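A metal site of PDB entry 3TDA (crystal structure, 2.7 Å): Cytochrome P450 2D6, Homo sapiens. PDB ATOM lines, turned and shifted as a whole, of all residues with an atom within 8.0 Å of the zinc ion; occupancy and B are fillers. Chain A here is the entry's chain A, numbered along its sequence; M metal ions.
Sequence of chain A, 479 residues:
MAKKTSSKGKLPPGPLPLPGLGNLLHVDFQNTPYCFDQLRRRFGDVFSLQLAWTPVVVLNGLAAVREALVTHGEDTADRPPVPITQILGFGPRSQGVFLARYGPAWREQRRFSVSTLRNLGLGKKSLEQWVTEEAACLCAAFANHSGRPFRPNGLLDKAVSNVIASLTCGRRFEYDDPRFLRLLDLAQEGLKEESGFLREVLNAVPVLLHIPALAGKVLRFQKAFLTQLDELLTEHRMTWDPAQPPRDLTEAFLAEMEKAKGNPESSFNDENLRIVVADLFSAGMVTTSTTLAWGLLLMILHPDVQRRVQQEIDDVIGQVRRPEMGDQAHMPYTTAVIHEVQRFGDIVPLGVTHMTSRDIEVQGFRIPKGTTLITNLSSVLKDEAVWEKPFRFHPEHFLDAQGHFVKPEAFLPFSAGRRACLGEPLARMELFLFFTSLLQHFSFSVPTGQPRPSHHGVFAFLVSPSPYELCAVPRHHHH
The side-chain carboxylate (OE1) of Glu 251 sits at hydrogen-bond distance from the backbone NH (N) of Arg 247 (3.1 Å).
OG1 of Thr 239 lies within hydrogen-bond range of O of His 236 (3.4 Å).
The side-chain carboxylate (OD1) of Asp 248 sits at hydrogen-bond distance from the backbone NH (N) of Thr 250 (3.3 Å).
The zinc ion is bound by OE2 of Glu 251 (1.8 Å), NE2 of His 236 (2.0 Å) and OD2 of Asp 248 (2.1 Å).
Of the 21 residues printed, 3 come within 4 Å of the zinc ion.
Along chain A the residues within 4 Å of the zinc ion span positions 236 to 251.
The nearest printed residue that does not touch the zinc ion is Arg 247 (4.4 Å).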
ATOM      1  N   ALA A 165      24.910   8.105  29.613  1.00  0.00           N
ATOM      2  CA  ALA A 165      25.042   7.064  28.588  1.00  0.00           C
ATOM      3  C   ALA A 165      23.815   6.149  28.664  1.00  0.00           C
ATOM      4  O   ALA A 165      23.262   5.755  27.643  1.00  0.00           O
ATOM      5  CB  ALA A 165      26.314   6.261  28.819  1.00  0.00           C
ATOM      6  N   SER A 166      23.396   5.801  29.877  1.00  0.00           N
ATOM      7  CA  SER A 166      22.231   4.938  30.081  1.00  0.00           C
ATOM      8  C   SER A 166      20.991   5.530  29.427  1.00  0.00           C
ATOM      9  O   SER A 166      20.220   4.842  28.779  1.00  0.00           O
ATOM     10  CB  SER A 166      21.948   4.747  31.587  1.00  0.00           C
ATOM     11  OG  SER A 166      20.730   4.046  31.806  1.00  0.00           O
ATOM     12  N   LEU A 167      20.814   6.833  29.631  1.00  0.00           N
ATOM     13  CA  LEU A 167      19.683   7.595  29.109  1.00  0.00           C
ATOM     14  C   LEU A 167      19.718   7.760  27.597  1.00  0.00           C
ATOM     15  O   LEU A 167      18.713   7.577  26.916  1.00  0.00           O
ATOM     16  CB  LEU A 167      19.657   8.984  29.754  1.00  0.00           C
ATOM     17  CG  LEU A 167      18.719   9.376  30.893  1.00  0.00           C
ATOM     18  CD1 LEU A 167      18.141   8.191  31.611  1.00  0.00           C
ATOM     19  CD2 LEU A 167      19.504  10.280  31.832  1.00  0.00           C
ATOM     20  N   THR A 168      20.883   8.102  27.070  1.00  0.00           N
ATOM     21  CA  THR A 168      21.051   8.311  25.648  1.00  0.00           C
ATOM     22  C   THR A 168      21.379   7.057  24.861  1.00  0.00           C
ATOM     23  O   THR A 168      20.717   6.747  23.868  1.00  0.00           O
ATOM     24  CB  THR A 168      22.155   9.349  25.366  1.00  0.00           C
ATOM     25  OG1 THR A 168      23.407   8.878  25.880  1.00  0.00           O
ATOM     26  CG2 THR A 168      21.829  10.652  26.064  1.00  0.00           C
ATOM     27  N   CYS A 169      22.384   6.319  25.316  1.00  0.00           N
ATOM     28  CA  CYS A 169      22.833   5.095  24.645  1.00  0.00           C
ATOM     29  C   CYS A 169      22.266   3.796  25.198  1.00  0.00           C
ATOM     30  O   CYS A 169      22.619   2.734  24.717  1.00  0.00           O
ATOM     31  CB  CYS A 169      24.360   5.047  24.685  1.00  0.00           C
ATOM     32  SG  CYS A 169      25.179   6.414  23.829  1.00  0.00           S
ATOM     33  N   GLY A 170      21.411   3.852  26.207  1.00  0.00           N
ATOM     34  CA  GLY A 170      20.846   2.638  26.771  1.00  0.00           C
ATOM     35  C   GLY A 170      21.818   1.643  27.443  1.00  0.00           C
ATOM     36  O   GLY A 170      21.487   0.494  27.623  1.00  0.00           O
ATOM     37  N   ARG A 171      23.009   2.075  27.844  1.00  0.00           N
ATOM     38  CA  ARG A 171      23.941   1.145  28.450  1.00  0.00           C
ATOM     39  C   ARG A 171      24.963   1.873  29.292  1.00  0.00           C
ATOM     40  O   ARG A 171      25.078   3.088  29.220  1.00  0.00           O
ATOM     41  CB  ARG A 171      24.701   0.382  27.368  1.00  0.00           C
ATOM     42  CG  ARG A 171      25.551   1.315  26.483  1.00  0.00           C
ATOM     43  CD  ARG A 171      26.558   0.565  25.677  1.00  0.00           C
ATOM     44  NE  ARG A 171      27.460  -0.190  26.554  1.00  0.00           N
ATOM     45  CZ  ARG A 171      28.413  -1.019  26.139  1.00  0.00           C
ATOM     46  NH1 ARG A 171      28.627  -1.217  24.849  1.00  0.00           N
ATOM     47  NH2 ARG A 171      29.164  -1.639  27.025  1.00  0.00           N
ATOM     48  N   HIS A 236      24.320   0.311  18.205  1.00  0.00           N
ATOM     49  CA  HIS A 236      22.982   0.524  18.747  1.00  0.00           C
ATOM     50  C   HIS A 236      21.911   0.382  17.688  1.00  0.00           C
ATOM     51  O   HIS A 236      20.841  -0.189  17.942  1.00  0.00           O
ATOM     52  CB  HIS A 236      22.891   1.907  19.405  1.00  0.00           C
ATOM     53  CG  HIS A 236      21.774   2.037  20.384  1.00  0.00           C
ATOM     54  ND1 HIS A 236      21.677   3.093  21.258  1.00  0.00           N
ATOM     55  CD2 HIS A 236      20.720   1.230  20.651  1.00  0.00           C
ATOM     56  CE1 HIS A 236      20.610   2.935  22.017  1.00  0.00           C
ATOM     57  NE2 HIS A 236      20.011   1.815  21.671  1.00  0.00           N
ATOM     58  N   ARG A 237      22.178   0.893  16.491  1.00  0.00           N
ATOM     59  CA  ARG A 237      21.198   0.794  15.424  1.00  0.00           C
ATOM     60  C   ARG A 237      20.951  -0.688  15.177  1.00  0.00           C
ATOM     61  O   ARG A 237      19.845  -1.089  14.786  1.00  0.00           O
ATOM     62  CB  ARG A 237      21.715   1.496  14.176  1.00  0.00           C
ATOM     63  CG  ARG A 237      20.713   1.590  13.027  1.00  0.00           C
ATOM     64  CD  ARG A 237      20.387   3.046  12.637  1.00  0.00           C
ATOM     65  NE  ARG A 237      21.568   3.923  12.592  1.00  0.00           N
ATOM     66  CZ  ARG A 237      21.523   5.191  12.163  1.00  0.00           C
ATOM     67  NH1 ARG A 237      20.375   5.711  11.743  1.00  0.00           N
ATOM     68  NH2 ARG A 237      22.633   5.932  12.156  1.00  0.00           N
ATOM     69  N   THR A 239      21.289  -3.283  17.591  1.00  0.00           N
ATOM     70  CA  THR A 239      20.609  -3.949  18.709  1.00  0.00           C
ATOM     71  C   THR A 239      19.189  -3.430  18.948  1.00  0.00           C
ATOM     72  O   THR A 239      18.359  -4.105  19.542  1.00  0.00           O
ATOM     73  CB  THR A 239      21.431  -3.794  20.031  1.00  0.00           C
ATOM     74  OG1 THR A 239      21.462  -2.408  20.421  1.00  0.00           O
ATOM     75  CG2 THR A 239      22.870  -4.285  19.830  1.00  0.00           C
ATOM     76  N   TRP A 240      18.907  -2.225  18.457  1.00  0.00           N
ATOM     77  CA  TRP A 240      17.596  -1.604  18.627  1.00  0.00           C
ATOM     78  C   TRP A 240      16.449  -2.513  18.195  1.00  0.00           C
ATOM     79  O   TRP A 240      16.502  -3.152  17.140  1.00  0.00           O
ATOM     80  CB  TRP A 240      17.553  -0.283  17.849  1.00  0.00           C
ATOM     81  CG  TRP A 240      16.227   0.382  17.797  1.00  0.00           C
ATOM     82  CD1 TRP A 240      15.332   0.523  18.837  1.00  0.00           C
ATOM     83  CD2 TRP A 240      15.656   1.078  16.683  1.00  0.00           C
ATOM     84  NE1 TRP A 240      14.238   1.260  18.428  1.00  0.00           N
ATOM     85  CE2 TRP A 240      14.412   1.619  17.117  1.00  0.00           C
ATOM     86  CE3 TRP A 240      16.062   1.298  15.359  1.00  0.00           C
ATOM     87  CZ2 TRP A 240      13.574   2.369  16.275  1.00  0.00           C
ATOM     88  CZ3 TRP A 240      15.223   2.062  14.521  1.00  0.00           C
ATOM     89  CH2 TRP A 240      14.008   2.582  14.985  1.00  0.00           C
ATOM     90  N   ASP A 241      15.426  -2.580  19.039  1.00  0.00           N
ATOM     91  CA  ASP A 241      14.226  -3.366  18.781  1.00  0.00           C
ATOM     92  C   ASP A 241      13.076  -2.356  18.598  1.00  0.00           C
ATOM     93  O   ASP A 241      12.467  -1.908  19.568  1.00  0.00           O
ATOM     94  CB  ASP A 241      13.936  -4.300  19.949  1.00  0.00           C
ATOM     95  CG  ASP A 241      12.716  -5.186  19.713  1.00  0.00           C
ATOM     96  OD1 ASP A 241      12.428  -6.018  20.599  1.00  0.00           O
ATOM     97  OD2 ASP A 241      12.062  -5.052  18.653  1.00  0.00           O
ATOM     98  N   PRO A 245       8.740  -0.054  22.871  1.00  0.00           N
ATOM     99  CA  PRO A 245       8.828   1.388  23.100  1.00  0.00           C
ATOM    100  C   PRO A 245      10.307   1.727  23.337  1.00  0.00           C
ATOM    101  O   PRO A 245      11.025   0.936  23.956  1.00  0.00           O
ATOM    102  CB  PRO A 245       7.979   1.589  24.360  1.00  0.00           C
ATOM    103  CG  PRO A 245       6.976   0.452  24.278  1.00  0.00           C
ATOM    104  CD  PRO A 245       7.829  -0.694  23.828  1.00  0.00           C
ATOM    105  N   PRO A 246      10.771   2.898  22.877  1.00  0.00           N
ATOM    106  CA  PRO A 246      12.171   3.274  23.062  1.00  0.00           C
ATOM    107  C   PRO A 246      12.688   3.134  24.494  1.00  0.00           C
ATOM    108  O   PRO A 246      12.018   3.536  25.430  1.00  0.00           O
ATOM    109  CB  PRO A 246      12.203   4.713  22.570  1.00  0.00           C
ATOM    110  CG  PRO A 246      11.209   4.700  21.477  1.00  0.00           C
ATOM    111  CD  PRO A 246      10.062   3.934  22.111  1.00  0.00           C
ATOM    112  N   ARG A 247      13.867   2.551  24.660  1.00  0.00           N
ATOM    113  CA  ARG A 247      14.477   2.377  25.974  1.00  0.00           C
ATOM    114  C   ARG A 247      15.375   3.568  26.300  1.00  0.00           C
ATOM    115  O   ARG A 247      15.733   3.798  27.449  1.00  0.00           O
ATOM    116  CB  ARG A 247      15.393   1.158  26.008  1.00  0.00           C
ATOM    117  CG  ARG A 247      14.821  -0.158  25.604  1.00  0.00           C
ATOM    118  CD  ARG A 247      15.563  -1.264  26.363  1.00  0.00           C
ATOM    119  NE  ARG A 247      16.987  -0.947  26.435  1.00  0.00           N
ATOM    120  CZ  ARG A 247      17.656  -0.665  27.555  1.00  0.00           C
ATOM    121  NH1 ARG A 247      17.045  -0.655  28.717  1.00  0.00           N
ATOM    122  NH2 ARG A 247      18.948  -0.358  27.482  1.00  0.00           N
ATOM    123  N   ASP A 248      15.788   4.293  25.276  1.00  0.00           N
ATOM    124  CA  ASP A 248      16.700   5.402  25.487  1.00  0.00           C
ATOM    125  C   ASP A 248      16.415   6.494  24.484  1.00  0.00           C
ATOM    126  O   ASP A 248      15.562   6.331  23.628  1.00  0.00           O
ATOM    127  CB  ASP A 248      18.126   4.896  25.348  1.00  0.00           C
ATOM    128  CG  ASP A 248      18.301   3.986  24.146  1.00  0.00           C
ATOM    129  OD1 ASP A 248      18.284   4.472  22.993  1.00  0.00           O
ATOM    130  OD2 ASP A 248      18.434   2.765  24.359  1.00  0.00           O
ATOM    131  N   LEU A 249      17.152   7.593  24.607  1.00  0.00           N
ATOM    132  CA  LEU A 249      16.964   8.736  23.719  1.00  0.00           C
ATOM    133  C   LEU A 249      17.402   8.439  22.280  1.00  0.00           C
ATOM    134  O   LEU A 249      16.819   8.963  21.343  1.00  0.00           O
ATOM    135  CB  LEU A 249      17.707   9.956  24.257  1.00  0.00           C
ATOM    136  CG  LEU A 249      17.437  11.266  23.507  1.00  0.00           C
ATOM    137  CD1 LEU A 249      17.273  12.402  24.494  1.00  0.00           C
ATOM    138  CD2 LEU A 249      18.565  11.571  22.538  1.00  0.00           C
ATOM    139  N   THR A 250      18.431   7.622  22.109  1.00  0.00           N
ATOM    140  CA  THR A 250      18.867   7.290  20.762  1.00  0.00           C
ATOM    141  C   THR A 250      17.755   6.517  20.032  1.00  0.00           C
ATOM    142  O   THR A 250      17.508   6.730  18.844  1.00  0.00           O
ATOM    143  CB  THR A 250      20.170   6.463  20.817  1.00  0.00           C
ATOM    144  OG1 THR A 250      21.246   7.303  21.251  1.00  0.00           O
ATOM    145  CG2 THR A 250      20.507   5.875  19.452  1.00  0.00           C
ATOM    146  N   GLU A 251      17.074   5.614  20.732  1.00  0.00           N
ATOM    147  CA  GLU A 251      16.011   4.854  20.082  1.00  0.00           C
ATOM    148  C   GLU A 251      14.851   5.802  19.784  1.00  0.00           C
ATOM    149  O   GLU A 251      14.315   5.787  18.672  1.00  0.00           O
ATOM    150  CB  GLU A 251      15.529   3.690  20.947  1.00  0.00           C
ATOM    151  CG  GLU A 251      16.464   2.493  20.923  1.00  0.00           C
ATOM    152  CD  GLU A 251      16.081   1.425  21.956  1.00  0.00           C
ATOM    153  OE1 GLU A 251      14.860   1.147  22.106  1.00  0.00           O
ATOM    154  OE2 GLU A 251      16.996   0.859  22.621  1.00  0.00           O
ATOM    155  N   ALA A 252      14.492   6.634  20.756  1.00  0.00           N
ATOM    156  CA  ALA A 252      13.400   7.568  20.532  1.00  0.00           C
ATOM    157  C   ALA A 252      13.732   8.391  19.289  1.00  0.00           C
ATOM    158  O   ALA A 252      12.879   8.533  18.400  1.00  0.00           O
ATOM    159  CB  ALA A 252      13.219   8.472  21.729  1.00  0.00           C
ATOM    160  N   LEU A 254      15.742   7.664  16.794  1.00  0.00           N
ATOM    161  CA  LEU A 254      15.654   6.764  15.648  1.00  0.00           C
ATOM    162  C   LEU A 254      14.212   6.598  15.175  1.00  0.00           C
ATOM    163  O   LEU A 254      13.933   6.735  13.994  1.00  0.00           O
ATOM    164  CB  LEU A 254      16.234   5.380  15.971  1.00  0.00           C
ATOM    165  CG  LEU A 254      17.751   5.277  16.182  1.00  0.00           C
ATOM    166  CD1 LEU A 254      18.109   3.899  16.684  1.00  0.00           C
ATOM    167  CD2 LEU A 254      18.487   5.599  14.898  1.00  0.00           C
HETATM  168 ZN    ZN M   1      18.717   1.208  23.025  1.00  0.00          ZN
